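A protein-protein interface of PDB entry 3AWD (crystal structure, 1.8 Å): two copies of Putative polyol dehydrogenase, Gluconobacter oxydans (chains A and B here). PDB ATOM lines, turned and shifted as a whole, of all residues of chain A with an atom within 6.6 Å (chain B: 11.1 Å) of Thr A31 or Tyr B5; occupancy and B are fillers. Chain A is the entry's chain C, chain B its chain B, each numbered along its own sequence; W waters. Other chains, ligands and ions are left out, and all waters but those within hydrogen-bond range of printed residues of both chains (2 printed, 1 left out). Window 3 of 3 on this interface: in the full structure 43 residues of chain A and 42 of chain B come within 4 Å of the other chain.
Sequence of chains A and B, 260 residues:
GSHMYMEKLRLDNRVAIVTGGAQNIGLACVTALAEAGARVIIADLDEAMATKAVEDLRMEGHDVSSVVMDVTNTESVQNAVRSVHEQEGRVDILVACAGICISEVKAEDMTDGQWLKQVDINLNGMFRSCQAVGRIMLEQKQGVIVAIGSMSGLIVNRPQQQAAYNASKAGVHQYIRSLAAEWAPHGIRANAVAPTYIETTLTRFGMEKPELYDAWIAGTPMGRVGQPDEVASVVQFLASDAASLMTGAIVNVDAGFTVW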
ATOM      1  N   GLY A  26     -27.490 -12.744  -5.578  1.00  0.00           N
ATOM      2  CA  GLY A  26     -26.967 -11.528  -6.241  1.00  0.00           C
ATOM      3  C   GLY A  26     -26.085 -10.697  -5.316  1.00  0.00           C
ATOM      4  O   GLY A  26     -24.969 -10.323  -5.675  1.00  0.00           O
ATOM      5  N   LEU A  27     -26.584 -10.443  -4.107  1.00  0.00           N
ATOM      6  CA  LEU A  27     -25.857  -9.620  -3.135  1.00  0.00           C
ATOM      7  C   LEU A  27     -24.560 -10.278  -2.662  1.00  0.00           C
ATOM      8  O   LEU A  27     -23.546  -9.588  -2.476  1.00  0.00           O
ATOM      9  CB  LEU A  27     -26.753  -9.273  -1.939  1.00  0.00           C
ATOM     10  CG  LEU A  27     -26.135  -8.375  -0.856  1.00  0.00           C
ATOM     11  CD1 LEU A  27     -25.550  -7.067  -1.434  1.00  0.00           C
ATOM     12  CD2 LEU A  27     -27.209  -8.052   0.192  1.00  0.00           C
ATOM     13  N   ALA A  28     -24.606 -11.604  -2.462  1.00  0.00           N
ATOM     14  CA  ALA A  28     -23.394 -12.374  -2.164  1.00  0.00           C
ATOM     15  C   ALA A  28     -22.387 -12.252  -3.301  1.00  0.00           C
ATOM     16  O   ALA A  28     -21.182 -12.068  -3.058  1.00  0.00           O
ATOM     17  CB  ALA A  28     -23.732 -13.862  -1.870  1.00  0.00           C
ATOM     18  N   CYS A  29     -22.863 -12.341  -4.543  1.00  0.00           N
ATOM     19  CA  CYS A  29     -21.950 -12.146  -5.691  1.00  0.00           C
ATOM     20  C   CYS A  29     -21.338 -10.745  -5.702  1.00  0.00           C
ATOM     21  O   CYS A  29     -20.135 -10.617  -5.883  1.00  0.00           O
ATOM     22  CB  CYS A  29     -22.638 -12.433  -7.014  1.00  0.00           C
ATOM     23  SG  CYS A  29     -23.046 -14.191  -7.200  1.00  0.00           S
ATOM     24  N   VAL A  30     -22.163  -9.711  -5.493  1.00  0.00           N
ATOM     25  CA  VAL A  30     -21.679  -8.315  -5.403  1.00  0.00           C
ATOM     26  C   VAL A  30     -20.551  -8.226  -4.358  1.00  0.00           C
ATOM     27  O   VAL A  30     -19.503  -7.641  -4.624  1.00  0.00           O
ATOM     28  CB  VAL A  30     -22.840  -7.342  -5.017  1.00  0.00           C
ATOM     29  CG1 VAL A  30     -22.323  -5.958  -4.604  1.00  0.00           C
ATOM     30  CG2 VAL A  30     -23.863  -7.217  -6.161  1.00  0.00           C
ATOM     31  N   THR A  31     -20.780  -8.833  -3.193  1.00  0.00           N
ATOM     32  CA  THR A  31     -19.826  -8.768  -2.072  1.00  0.00           C
ATOM     33  C   THR A  31     -18.493  -9.450  -2.437  1.00  0.00           C
ATOM     34  O   THR A  31     -17.406  -8.874  -2.221  1.00  0.00           O
ATOM     35  CB  THR A  31     -20.429  -9.399  -0.774  1.00  0.00           C
ATOM     36  OG1 THR A  31     -21.704  -8.806  -0.493  1.00  0.00           O
ATOM     37  CG2 THR A  31     -19.499  -9.173   0.410  1.00  0.00           C
ATOM     38  N   ALA A  32     -18.578 -10.652  -3.014  1.00  0.00           N
ATOM     39  CA  ALA A  32     -17.369 -11.400  -3.416  1.00  0.00           C
ATOM     40  C   ALA A  32     -16.570 -10.656  -4.468  1.00  0.00           C
ATOM     41  O   ALA A  32     -15.337 -10.552  -4.375  1.00  0.00           O
ATOM     42  CB  ALA A  32     -17.719 -12.837  -3.906  1.00  0.00           C
ATOM     43  N   LEU A  33     -17.269 -10.116  -5.460  1.00  0.00           N
ATOM     44  CA  LEU A  33     -16.619  -9.331  -6.493  1.00  0.00           C
ATOM     45  C   LEU A  33     -15.899  -8.126  -5.879  1.00  0.00           C
ATOM     46  O   LEU A  33     -14.740  -7.846  -6.217  1.00  0.00           O
ATOM     47  CB  LEU A  33     -17.636  -8.896  -7.561  1.00  0.00           C
ATOM     48  CG  LEU A  33     -18.234 -10.036  -8.401  1.00  0.00           C
ATOM     49  CD1 LEU A  33     -19.450  -9.531  -9.185  1.00  0.00           C
ATOM     50  CD2 LEU A  33     -17.207 -10.690  -9.340  1.00  0.00           C
ATOM     51  N   ALA A  34     -16.579  -7.430  -4.973  1.00  0.00           N
ATOM     52  CA  ALA A  34     -16.018  -6.214  -4.356  1.00  0.00           C
ATOM     53  C   ALA A  34     -14.794  -6.565  -3.498  1.00  0.00           C
ATOM     54  O   ALA A  34     -13.786  -5.865  -3.516  1.00  0.00           O
ATOM     55  CB  ALA A  34     -17.072  -5.499  -3.516  1.00  0.00           C
ATOM     56  N   GLU A  35     -14.887  -7.661  -2.753  1.00  0.00           N
ATOM     57  CA  GLU A  35     -13.755  -8.097  -1.928  1.00  0.00           C
ATOM     58  C   GLU A  35     -12.542  -8.452  -2.782  1.00  0.00           C
ATOM     59  O   GLU A  35     -11.406  -8.254  -2.357  1.00  0.00           O
ATOM     60  CB  GLU A  35     -14.156  -9.265  -1.027  1.00  0.00           C
ATOM     61  CG  GLU A  35     -15.042  -8.839   0.165  1.00  0.00           C
ATOM     62  CD  GLU A  35     -15.314  -9.970   1.166  1.00  0.00           C
ATOM     63  OE1 GLU A  35     -14.587 -10.977   1.158  1.00  0.00           O
ATOM     64  OE2 GLU A  35     -16.253  -9.834   1.986  1.00  0.00           O
ATOM     65  N   ALA A  36     -12.782  -8.946  -3.996  1.00  0.00           N
ATOM     66  CA  ALA A  36     -11.688  -9.194  -4.945  1.00  0.00           C
ATOM     67  C   ALA A  36     -11.131  -7.936  -5.623  1.00  0.00           C
ATOM     68  O   ALA A  36     -10.180  -8.027  -6.403  1.00  0.00           O
ATOM     69  CB  ALA A  36     -12.127 -10.227  -6.011  1.00  0.00           C
ATOM     70  N   VAL A  40     -18.369  -2.483  -8.359  1.00  0.00           N
ATOM     71  CA  VAL A  40     -19.572  -3.273  -8.613  1.00  0.00           C
ATOM     72  C   VAL A  40     -20.833  -2.416  -8.690  1.00  0.00           C
ATOM     73  O   VAL A  40     -21.018  -1.516  -7.870  1.00  0.00           O
ATOM     74  CB  VAL A  40     -19.783  -4.378  -7.534  1.00  0.00           C
ATOM     75  CG1 VAL A  40     -20.896  -5.312  -7.975  1.00  0.00           C
ATOM     76  CG2 VAL A  40     -18.487  -5.159  -7.281  1.00  0.00           C
ATOM     77  N   LEU A  57     -22.453  -1.801   1.992  1.00  0.00           N
ATOM     78  CA  LEU A  57     -21.189  -2.175   1.370  1.00  0.00           C
ATOM     79  C   LEU A  57     -20.171  -1.040   1.376  1.00  0.00           C
ATOM     80  O   LEU A  57     -18.984  -1.274   1.595  1.00  0.00           O
ATOM     81  CB  LEU A  57     -21.424  -2.710  -0.048  1.00  0.00           C
ATOM     82  CG  LEU A  57     -22.061  -4.119  -0.092  1.00  0.00           C
ATOM     83  CD1 LEU A  57     -22.863  -4.310  -1.360  1.00  0.00           C
ATOM     84  CD2 LEU A  57     -21.016  -5.198   0.048  1.00  0.00           C
ATOM     85  N   HIS A  62     -16.163  -0.815   0.421  1.00  0.00           N
ATOM     86  CA  HIS A  62     -16.299  -1.258  -0.974  1.00  0.00           C
ATOM     87  C   HIS A  62     -16.813  -0.188  -1.926  1.00  0.00           C
ATOM     88  O   HIS A  62     -17.574   0.709  -1.535  1.00  0.00           O
ATOM     89  CB  HIS A  62     -17.183  -2.505  -1.076  1.00  0.00           C
ATOM     90  CG  HIS A  62     -16.703  -3.639  -0.229  1.00  0.00           C
ATOM     91  ND1 HIS A  62     -15.400  -4.089  -0.261  1.00  0.00           N
ATOM     92  CD2 HIS A  62     -17.346  -4.411   0.676  1.00  0.00           C
ATOM     93  CE1 HIS A  62     -15.260  -5.088   0.590  1.00  0.00           C
ATOM     94  NE2 HIS A  62     -16.426  -5.303   1.175  1.00  0.00           N
ATOM     95  N   VAL A  64     -19.193   0.327  -4.483  1.00  0.00           N
ATOM     96  CA  VAL A  64     -20.432  -0.237  -4.994  1.00  0.00           C
ATOM     97  C   VAL A  64     -21.425   0.882  -5.251  1.00  0.00           C
ATOM     98  O   VAL A  64     -21.454   1.893  -4.540  1.00  0.00           O
ATOM     99  CB  VAL A  64     -21.021  -1.289  -4.028  1.00  0.00           C
ATOM    100  CG1 VAL A  64     -22.281  -1.941  -4.617  1.00  0.00           C
ATOM    101  CG2 VAL A  64     -19.959  -2.363  -3.688  1.00  0.00           C
ATOM    102  N   PRO A 228     -25.687 -18.659   0.272  1.00  0.00           N
ATOM    103  CA  PRO A 228     -25.364 -17.759  -0.853  1.00  0.00           C
ATOM    104  C   PRO A 228     -23.863 -17.561  -1.092  1.00  0.00           C
ATOM    105  O   PRO A 228     -23.417 -17.474  -2.246  1.00  0.00           O
ATOM    106  CB  PRO A 228     -25.991 -16.418  -0.417  1.00  0.00           C
ATOM    107  CG  PRO A 228     -27.165 -16.835   0.424  1.00  0.00           C
ATOM    108  CD  PRO A 228     -26.695 -18.076   1.180  1.00  0.00           C
ATOM    109  N   ASP A 229     -23.084 -17.496  -0.016  1.00  0.00           N
ATOM    110  CA  ASP A 229     -21.641 -17.256  -0.167  1.00  0.00           C
ATOM    111  C   ASP A 229     -20.931 -18.400  -0.914  1.00  0.00           C
ATOM    112  O   ASP A 229     -19.892 -18.180  -1.544  1.00  0.00           O
ATOM    113  CB  ASP A 229     -20.968 -16.985   1.193  1.00  0.00           C
ATOM    114  CG  ASP A 229     -20.854 -18.242   2.055  1.00  0.00           C
ATOM    115  OD1 ASP A 229     -21.865 -18.614   2.691  1.00  0.00           O
ATOM    116  OD2 ASP A 229     -19.754 -18.838   2.107  1.00  0.00           O
ATOM    117  N   GLU A 230     -21.500 -19.605  -0.850  1.00  0.00           N
ATOM    118  CA  GLU A 230     -20.908 -20.750  -1.527  1.00  0.00           C
ATOM    119  C   GLU A 230     -21.091 -20.675  -3.033  1.00  0.00           C
ATOM    120  O   GLU A 230     -20.231 -21.157  -3.794  1.00  0.00           O
ATOM    121  CB  GLU A 230     -21.474 -22.047  -0.992  1.00  0.00           C
ATOM    122  CG  GLU A 230     -21.277 -22.222   0.507  1.00  0.00           C
ATOM    123  CD  GLU A 230     -21.714 -23.587   0.943  1.00  0.00           C
ATOM    124  OE1 GLU A 230     -22.928 -23.753   1.160  1.00  0.00           O
ATOM    125  OE2 GLU A 230     -20.844 -24.489   1.064  1.00  0.00           O
ATOM    126  N   VAL A 231     -22.190 -20.062  -3.467  1.00  0.00           N
ATOM    127  CA  VAL A 231     -22.373 -19.798  -4.911  1.00  0.00           C
ATOM    128  C   VAL A 231     -21.501 -18.614  -5.357  1.00  0.00           C
ATOM    129  O   VAL A 231     -20.854 -18.652  -6.432  1.00  0.00           O
ATOM    130  CB  VAL A 231     -23.844 -19.552  -5.251  1.00  0.00           C
ATOM    131  CG1 VAL A 231     -23.998 -19.178  -6.727  1.00  0.00           C
ATOM    132  CG2 VAL A 231     -24.659 -20.801  -4.917  1.00  0.00           C
ATOM    133  N   ALA A 232     -21.478 -17.567  -4.534  1.00  0.00           N
ATOM    134  CA  ALA A 232     -20.701 -16.357  -4.837  1.00  0.00           C
ATOM    135  C   ALA A 232     -19.222 -16.675  -5.041  1.00  0.00           C
ATOM    136  O   ALA A 232     -18.560 -16.087  -5.919  1.00  0.00           O
ATOM    137  CB  ALA A 232     -20.888 -15.324  -3.735  1.00  0.00           C
ATOM    138  N   SER A 233     -18.689 -17.595  -4.227  1.00  0.00           N
ATOM    139  CA  SER A 233     -17.275 -17.984  -4.379  1.00  0.00           C
ATOM    140  C   SER A 233     -16.975 -18.539  -5.780  1.00  0.00           C
ATOM    141  O   SER A 233     -15.940 -18.207  -6.387  1.00  0.00           O
ATOM    142  CB  SER A 233     -16.867 -18.993  -3.305  1.00  0.00           C
ATOM    143  OG  SER A 233     -16.546 -18.330  -2.092  1.00  0.00           O
ATOM    144  N   GLN A 236     -17.282 -15.653  -8.454  1.00  0.00           N
ATOM    145  CA  GLN A 236     -16.103 -14.781  -8.417  1.00  0.00           C
ATOM    146  C   GLN A 236     -14.954 -15.483  -9.127  1.00  0.00           C
ATOM    147  O   GLN A 236     -14.242 -14.876  -9.924  1.00  0.00           O
ATOM    148  CB  GLN A 236     -15.746 -14.424  -6.956  1.00  0.00           C
ATOM    149  CG  GLN A 236     -14.603 -13.347  -6.810  1.00  0.00           C
ATOM    150  CD  GLN A 236     -13.213 -13.926  -7.019  1.00  0.00           C
ATOM    151  OE1 GLN A 236     -12.935 -15.055  -6.606  1.00  0.00           O
ATOM    152  NE2 GLN A 236     -12.331 -13.161  -7.685  1.00  0.00           N
ATOM    153  N   MET B   4     -13.532 -12.242   3.959  1.00  0.00           N
ATOM    154  CA  MET B   4     -13.900 -13.683   4.030  1.00  0.00           C
ATOM    155  C   MET B   4     -13.702 -14.393   2.689  1.00  0.00           C
ATOM    156  O   MET B   4     -13.147 -15.500   2.664  1.00  0.00           O
ATOM    157  CB  MET B   4     -15.325 -13.877   4.579  1.00  0.00           C
ATOM    158  CG  MET B   4     -15.958 -15.262   4.299  1.00  0.00           C
ATOM    159  SD  MET B   4     -17.376 -15.266   3.149  1.00  0.00           S
ATOM    160  CE  MET B   4     -18.788 -15.294   4.253  1.00  0.00           C
ATOM    161  N   TYR B   5     -14.138 -13.780   1.584  1.00  0.00           N
ATOM    162  CA  TYR B   5     -14.121 -14.501   0.293  1.00  0.00           C
ATOM    163  C   TYR B   5     -12.705 -14.862  -0.151  1.00  0.00           C
ATOM    164  O   TYR B   5     -12.444 -15.987  -0.570  1.00  0.00           O
ATOM    165  CB  TYR B   5     -14.877 -13.751  -0.819  1.00  0.00           C
ATOM    166  CG  TYR B   5     -16.388 -13.852  -0.693  1.00  0.00           C
ATOM    167  CD1 TYR B   5     -17.058 -15.014  -1.097  1.00  0.00           C
ATOM    168  CD2 TYR B   5     -17.145 -12.787  -0.177  1.00  0.00           C
ATOM    169  CE1 TYR B   5     -18.436 -15.119  -0.987  1.00  0.00           C
ATOM    170  CE2 TYR B   5     -18.546 -12.875  -0.061  1.00  0.00           C
ATOM    171  CZ  TYR B   5     -19.181 -14.048  -0.475  1.00  0.00           C
ATOM    172  OH  TYR B   5     -20.548 -14.175  -0.374  1.00  0.00           O
ATOM    173  N   MET B   6     -11.781 -13.911  -0.046  1.00  0.00           N
ATOM    174  CA  MET B   6     -10.419 -14.180  -0.509  1.00  0.00           C
ATOM    175  C   MET B   6      -9.726 -15.204   0.404  1.00  0.00           C
ATOM    176  O   MET B   6      -8.948 -16.030  -0.070  1.00  0.00           O
ATOM    177  CB  MET B   6      -9.604 -12.878  -0.619  1.00  0.00           C
ATOM    178  CG  MET B   6     -10.110 -11.879  -1.682  1.00  0.00           C
ATOM    179  SD  MET B   6     -10.199 -12.511  -3.373  1.00  0.00           S
ATOM    180  CE  MET B   6     -11.844 -13.162  -3.427  1.00  0.00           C
ATOM    181  N   GLU B   7     -10.030 -15.154   1.701  1.00  0.00           N
ATOM    182  CA  GLU B   7      -9.447 -16.107   2.668  1.00  0.00           C
ATOM    183  C   GLU B   7      -9.834 -17.562   2.373  1.00  0.00           C
ATOM    184  O   GLU B   7      -9.073 -18.495   2.688  1.00  0.00           O
ATOM    185  CB  GLU B   7      -9.829 -15.734   4.106  1.00  0.00           C
ATOM    186  CG  GLU B   7      -9.104 -14.507   4.668  1.00  0.00           C
ATOM    187  CD  GLU B   7      -9.196 -14.410   6.213  1.00  0.00           C
ATOM    188  OE1 GLU B   7     -10.160 -14.970   6.815  1.00  0.00           O
ATOM    189  OE2 GLU B   7      -8.294 -13.773   6.827  1.00  0.00           O
ATOM    190  N   LYS B   8     -11.006 -17.767   1.765  1.00  0.00           N
ATOM    191  CA  LYS B   8     -11.468 -19.137   1.457  1.00  0.00           C
ATOM    192  C   LYS B   8     -10.559 -19.862   0.481  1.00  0.00           C
ATOM    193  O   LYS B   8     -10.596 -21.102   0.377  1.00  0.00           O
ATOM    194  CB  LYS B   8     -12.872 -19.121   0.846  1.00  0.00           C
ATOM    195  CG  LYS B   8     -14.022 -18.802   1.795  1.00  0.00           C
ATOM    196  CD  LYS B   8     -15.273 -19.025   0.932  1.00  0.00           C
ATOM    197  CE  LYS B   8     -16.539 -18.550   1.519  1.00  0.00           C
ATOM    198  NZ  LYS B   8     -17.641 -18.873   0.535  1.00  0.00           N
ATOM    199  N   LEU B   9      -9.776 -19.093  -0.267  1.00  0.00           N
ATOM    200  CA  LEU B   9      -8.912 -19.648  -1.303  1.00  0.00           C
ATOM    201  C   LEU B   9      -7.578 -20.180  -0.744  1.00  0.00           C
ATOM    202  O   LEU B   9      -6.846 -20.869  -1.449  1.00  0.00           O
ATOM    203  CB  LEU B   9      -8.708 -18.605  -2.425  1.00  0.00           C
ATOM    204  CG  LEU B   9     -10.075 -18.270  -3.092  1.00  0.00           C
ATOM    205  CD1 LEU B   9     -10.136 -16.856  -3.637  1.00  0.00           C
ATOM    206  CD2 LEU B   9     -10.362 -19.275  -4.197  1.00  0.00           C
ATOM    207  N   ARG B  10      -7.277 -19.872   0.521  1.00  0.00           N
ATOM    208  CA  ARG B  10      -5.978 -20.205   1.127  1.00  0.00           C
ATOM    209  C   ARG B  10      -5.936 -21.666   1.569  1.00  0.00           C
ATOM    210  O   ARG B  10      -6.954 -22.233   1.977  1.00  0.00           O
ATOM    211  CB  ARG B  10      -5.691 -19.302   2.344  1.00  0.00           C
ATOM    212  CG  ARG B  10      -5.455 -17.815   2.003  1.00  0.00           C
ATOM    213  CD  ARG B  10      -4.226 -17.585   1.146  1.00  0.00           C
ATOM    214  NE  ARG B  10      -2.988 -18.102   1.745  1.00  0.00           N
ATOM    215  CZ  ARG B  10      -1.819 -18.124   1.108  1.00  0.00           C
ATOM    216  NH1 ARG B  10      -1.743 -17.668  -0.135  1.00  0.00           N
ATOM    217  NH2 ARG B  10      -0.738 -18.619   1.691  1.00  0.00           N
ATOM    218  N   LEU B  11      -4.753 -22.266   1.491  1.00  0.00           N
ATOM    219  CA  LEU B  11      -4.575 -23.670   1.895  1.00  0.00           C
ATOM    220  C   LEU B  11      -3.454 -23.842   2.940  1.00  0.00           C
ATOM    221  O   LEU B  11      -2.804 -24.898   3.019  1.00  0.00           O
ATOM    222  CB  LEU B  11      -4.267 -24.512   0.656  1.00  0.00           C
ATOM    223  CG  LEU B  11      -5.304 -24.557  -0.476  1.00  0.00           C
ATOM    224  CD1 LEU B  11      -4.736 -25.352  -1.651  1.00  0.00           C
ATOM    225  CD2 LEU B  11      -6.626 -25.181  -0.003  1.00  0.00           C
ATOM    226  N   ARG B  14      -2.064 -27.034   4.942  1.00  0.00           N
ATOM    227  CA  ARG B  14      -2.735 -28.254   4.527  1.00  0.00           C
ATOM    228  C   ARG B  14      -1.746 -29.133   3.773  1.00  0.00           C
ATOM    229  O   ARG B  14      -0.871 -28.623   3.073  1.00  0.00           O
ATOM    230  CB  ARG B  14      -3.961 -27.940   3.666  1.00  0.00           C
ATOM    231  CG  ARG B  14      -4.949 -27.043   4.436  1.00  0.00           C
ATOM    232  CD  ARG B  14      -6.211 -26.736   3.663  1.00  0.00           C
ATOM    233  NE  ARG B  14      -7.023 -25.768   4.421  1.00  0.00           N
ATOM    234  CZ  ARG B  14      -8.309 -25.497   4.180  1.00  0.00           C
ATOM    235  NH1 ARG B  14      -8.974 -26.127   3.207  1.00  0.00           N
ATOM    236  NH2 ARG B  14      -8.937 -24.606   4.938  1.00  0.00           N
ATOM    237  N   GLN B 236      -6.675 -25.888  -7.970  1.00  0.00           N
ATOM    238  CA  GLN B 236      -6.426 -25.220  -6.688  1.00  0.00           C
ATOM    239  C   GLN B 236      -7.734 -24.713  -6.092  1.00  0.00           C
ATOM    240  O   GLN B 236      -7.990 -24.898  -4.890  1.00  0.00           O
ATOM    241  CB  GLN B 236      -5.414 -24.068  -6.867  1.00  0.00           C
ATOM    242  CG  GLN B 236      -4.927 -23.438  -5.535  1.00  0.00           C
ATOM    243  CD  GLN B 236      -5.939 -22.442  -4.948  1.00  0.00           C
ATOM    244  OE1 GLN B 236      -6.598 -21.711  -5.680  1.00  0.00           O
ATOM    245  NE2 GLN B 236      -6.048 -22.416  -3.612  1.00  0.00           N
ATOM    246  N   PHE B 237      -8.574 -24.113  -6.936  1.00  0.00           N
ATOM    247  CA  PHE B 237      -9.886 -23.659  -6.477  1.00  0.00           C
ATOM    248  C   PHE B 237     -10.724 -24.809  -5.887  1.00  0.00           C
ATOM    249  O   PHE B 237     -11.266 -24.711  -4.788  1.00  0.00           O
ATOM    250  CB  PHE B 237     -10.663 -22.956  -7.603  1.00  0.00           C
ATOM    251  CG  PHE B 237     -12.062 -22.546  -7.186  1.00  0.00           C
ATOM    252  CD1 PHE B 237     -12.261 -21.402  -6.427  1.00  0.00           C
ATOM    253  CD2 PHE B 237     -13.159 -23.337  -7.520  1.00  0.00           C
ATOM    254  CE1 PHE B 237     -13.542 -21.017  -6.027  1.00  0.00           C
ATOM    255  CE2 PHE B 237     -14.462 -22.979  -7.115  1.00  0.00           C
ATOM    256  CZ  PHE B 237     -14.638 -21.816  -6.358  1.00  0.00           C
ATOM    257  N   SER B 240      -9.897 -25.963  -2.484  1.00  0.00           N
ATOM    258  CA  SER B 240     -10.027 -24.962  -1.419  1.00  0.00           C
ATOM    259  C   SER B 240     -11.447 -24.927  -0.850  1.00  0.00           C
ATOM    260  O   SER B 240     -12.392 -25.443  -1.480  1.00  0.00           O
ATOM    261  CB  SER B 240      -9.655 -23.568  -1.935  1.00  0.00           C
ATOM    262  OG  SER B 240     -10.746 -23.014  -2.671  1.00  0.00           O
ATOM    263  N   ASP B 241     -11.592 -24.295   0.324  1.00  0.00           N
ATOM    264  CA  ASP B 241     -12.916 -24.100   0.938  1.00  0.00           C
ATOM    265  C   ASP B 241     -13.853 -23.216   0.118  1.00  0.00           C
ATOM    266  O   ASP B 241     -15.059 -23.213   0.363  1.00  0.00           O
ATOM    267  CB  ASP B 241     -12.801 -23.529   2.361  1.00  0.00           C
ATOM    268  CG  ASP B 241     -12.052 -24.463   3.315  1.00  0.00           C
ATOM    269  OD1 ASP B 241     -11.807 -25.635   2.954  1.00  0.00           O
ATOM    270  OD2 ASP B 241     -11.679 -23.982   4.412  1.00  0.00           O
ATOM    271  N   ALA B 242     -13.307 -22.452  -0.827  1.00  0.00           N
ATOM    272  CA  ALA B 242     -14.150 -21.677  -1.735  1.00  0.00           C
ATOM    273  C   ALA B 242     -15.119 -22.580  -2.524  1.00  0.00           C
ATOM    274  O   ALA B 242     -16.213 -22.147  -2.902  1.00  0.00           O
ATOM    275  CB  ALA B 242     -13.289 -20.837  -2.698  1.00  0.00           C
ATOM    276  N   ALA B 243     -14.693 -23.816  -2.786  1.00  0.00           N
ATOM    277  CA  ALA B 243     -15.497 -24.818  -3.507  1.00  0.00           C
ATOM    278  C   ALA B 243     -16.313 -25.725  -2.550  1.00  0.00           C
ATOM    279  O   ALA B 243     -16.653 -26.865  -2.882  1.00  0.00           O
ATOM    280  CB  ALA B 243     -14.574 -25.661  -4.405  1.00  0.00           C
ATOM    281  N   SER B 244     -16.632 -25.209  -1.358  1.00  0.00           N
ATOM    282  CA  SER B 244     -17.291 -25.995  -0.304  1.00  0.00           C
ATOM    283  C   SER B 244     -18.619 -26.626  -0.721  1.00  0.00           C
ATOM    284  O   SER B 244     -19.002 -27.651  -0.173  1.00  0.00           O
ATOM    285  CB  SER B 244     -17.513 -25.159   0.971  1.00  0.00           C
ATOM    286  OG  SER B 244     -18.330 -24.028   0.692  1.00  0.00           O
ATOM    287  N   LEU B 245     -19.321 -26.014  -1.670  1.00  0.00           N
ATOM    288  CA  LEU B 245     -20.611 -26.572  -2.105  1.00  0.00           C
ATOM    289  C   LEU B 245     -20.466 -27.537  -3.306  1.00  0.00           C
ATOM    290  O   LEU B 245     -21.443 -28.150  -3.754  1.00  0.00           O
ATOM    291  CB  LEU B 245     -21.639 -25.458  -2.366  1.00  0.00           C
ATOM    292  CG  LEU B 245     -23.113 -25.866  -2.493  1.00  0.00           C
ATOM    293  CD1 LEU B 245     -23.596 -26.561  -1.208  1.00  0.00           C
ATOM    294  CD2 LEU B 245     -23.972 -24.645  -2.801  1.00  0.00           C
HETATM  295  O   HOH W   1     -14.211 -17.123  -2.416  1.00  0.00           O
HETATM  296  O   HOH W   2     -18.694 -23.559  -3.328  1.00  0.00           O
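The backbone NH (N) of Met B4 sits at hydrogen-bond distance from the side-chain carboxylate (OE1) of Glu A35, 3.2 Å away.
The backbone carbonyl oxygen of Ala A28 lies within hydrogen-bond range of the side-chain hydroxyl of Tyr B5 (3.5 Å).
The side-chain carboxylate (OE1) of Glu A35 is in hydrogen-bond range of the backbone NH (N) of Tyr B5, at 2.9 Å.
The side-chain amino group (NZ) of Lys B8 is in salt-bridge range of the side-chain carboxylate (OD2) of Asp A229.
The side-chain amino group (NZ) of Lys B8 lies within hydrogen-bond range of the side-chain hydroxyl (OG) of Ser A233, at 2.9 Å.
OE2 of Glu A230 lies within hydrogen-bond range of OG of Ser B244, at 2.6 Å.
The side-chain carboxylate of Glu A230 is in hydrogen-bond range of the backbone NH of Leu B245 (3.5 Å).
The backbone carbonyl oxygen (O) of Lys B8 sits at hydrogen-bond distance from the backbone NH (N) of Ala B242 (3.3 Å).
OG of Ser B240 is in hydrogen-bond range of O of Phe B237, 2.8 Å away.
The side-chain hydroxyl (OG) of Ser A233 sits at hydrogen-bond distance from the backbone carbonyl oxygen (O) of Asp A229 (3.4 Å).
Among the printed residues, merely in contact across the chains: Thr A31 with Tyr B5, Ala A32 with Tyr B5, Glu A35 with Met B6, Ala A36 with Met B6, Asp A229 with Tyr B5, Ala A232 with Tyr B5, Ser A233 with Tyr B5, Ser A233 with Phe B237, Ser A233 with Ala B242 and Gln A236 with Met B6.
Thr A31 touches just one residue of chain B: Tyr B5 (3.9 Å).
Of the printed residues of chain A, Tyr B5 touches Ala A28, Thr A31, Ala A32, Glu A35, Asp A229, Ala A232 and Ser A233.
No residue of chain B comes within 4 Å of Leu A27.
Ala A28 touches just one residue of chain B: Tyr B5.
No residue of chain B comes within 4 Å of Val A30.
Ala A32 touches one residue of chain B.
No residue of chain B comes within 4 Å of Ala A34.
Glu A35 touches just these residues of chain B: Met B4, Tyr B5 and Met B6.
Ala A232 touches just one residue of chain B: Tyr B5.
Printed residues of chain A within 4 Å of Phe B237: Ser A233.
Printed residues of chain A within 4 Å of Met B4: Glu A35.
Gly A26 touches none of the printed residues of chain B.
His A62 touches none of the printed residues of chain B.
Of the 22 printed residues of chain A, 10 touch a printed residue of chain B.
Hydrophobic or aromatic side chains of chain A that line the printed part of chain B: Ala A28, Ala A32, Ala A36 and Ala A232.
Printed residues of chain B that touch a printed residue of chain A: Met B4, Tyr B5, Met B6, Lys B8, Phe B237, Ala B242, Ser B244 and Leu B245.
Hydrophobic or aromatic side chains of chain B within 4 Å of the printed part of chain A: Tyr B5, Met B6, Phe B237 and Leu B245.
Along chain B the printed residues that touch a printed residue of chain A span positions 4 to 245.
Among the printed residues, 17 pairs touch across the chains.
Among the printed residues, Asp or Glu carboxylates within 4 Å of a Lys or Arg side-chain nitrogen of the other chain: Asp A229 with Lys B8 (2.6 Å).
Position printed for both chains: 236.
Of the 17 pairs that touch across the chains among the printed residues, none has its exchanged pair printed and touching as well.
Water W1 lies within hydrogen-bond range of the side-chain hydroxyl of Ser A233 (2.6 Å) and the backbone carbonyl oxygen of Tyr B5 (2.8 Å).
Water W2 lies within hydrogen-bond range of O of Ala B242, O of Glu A230, N of Leu B245 and N of Ser B244.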
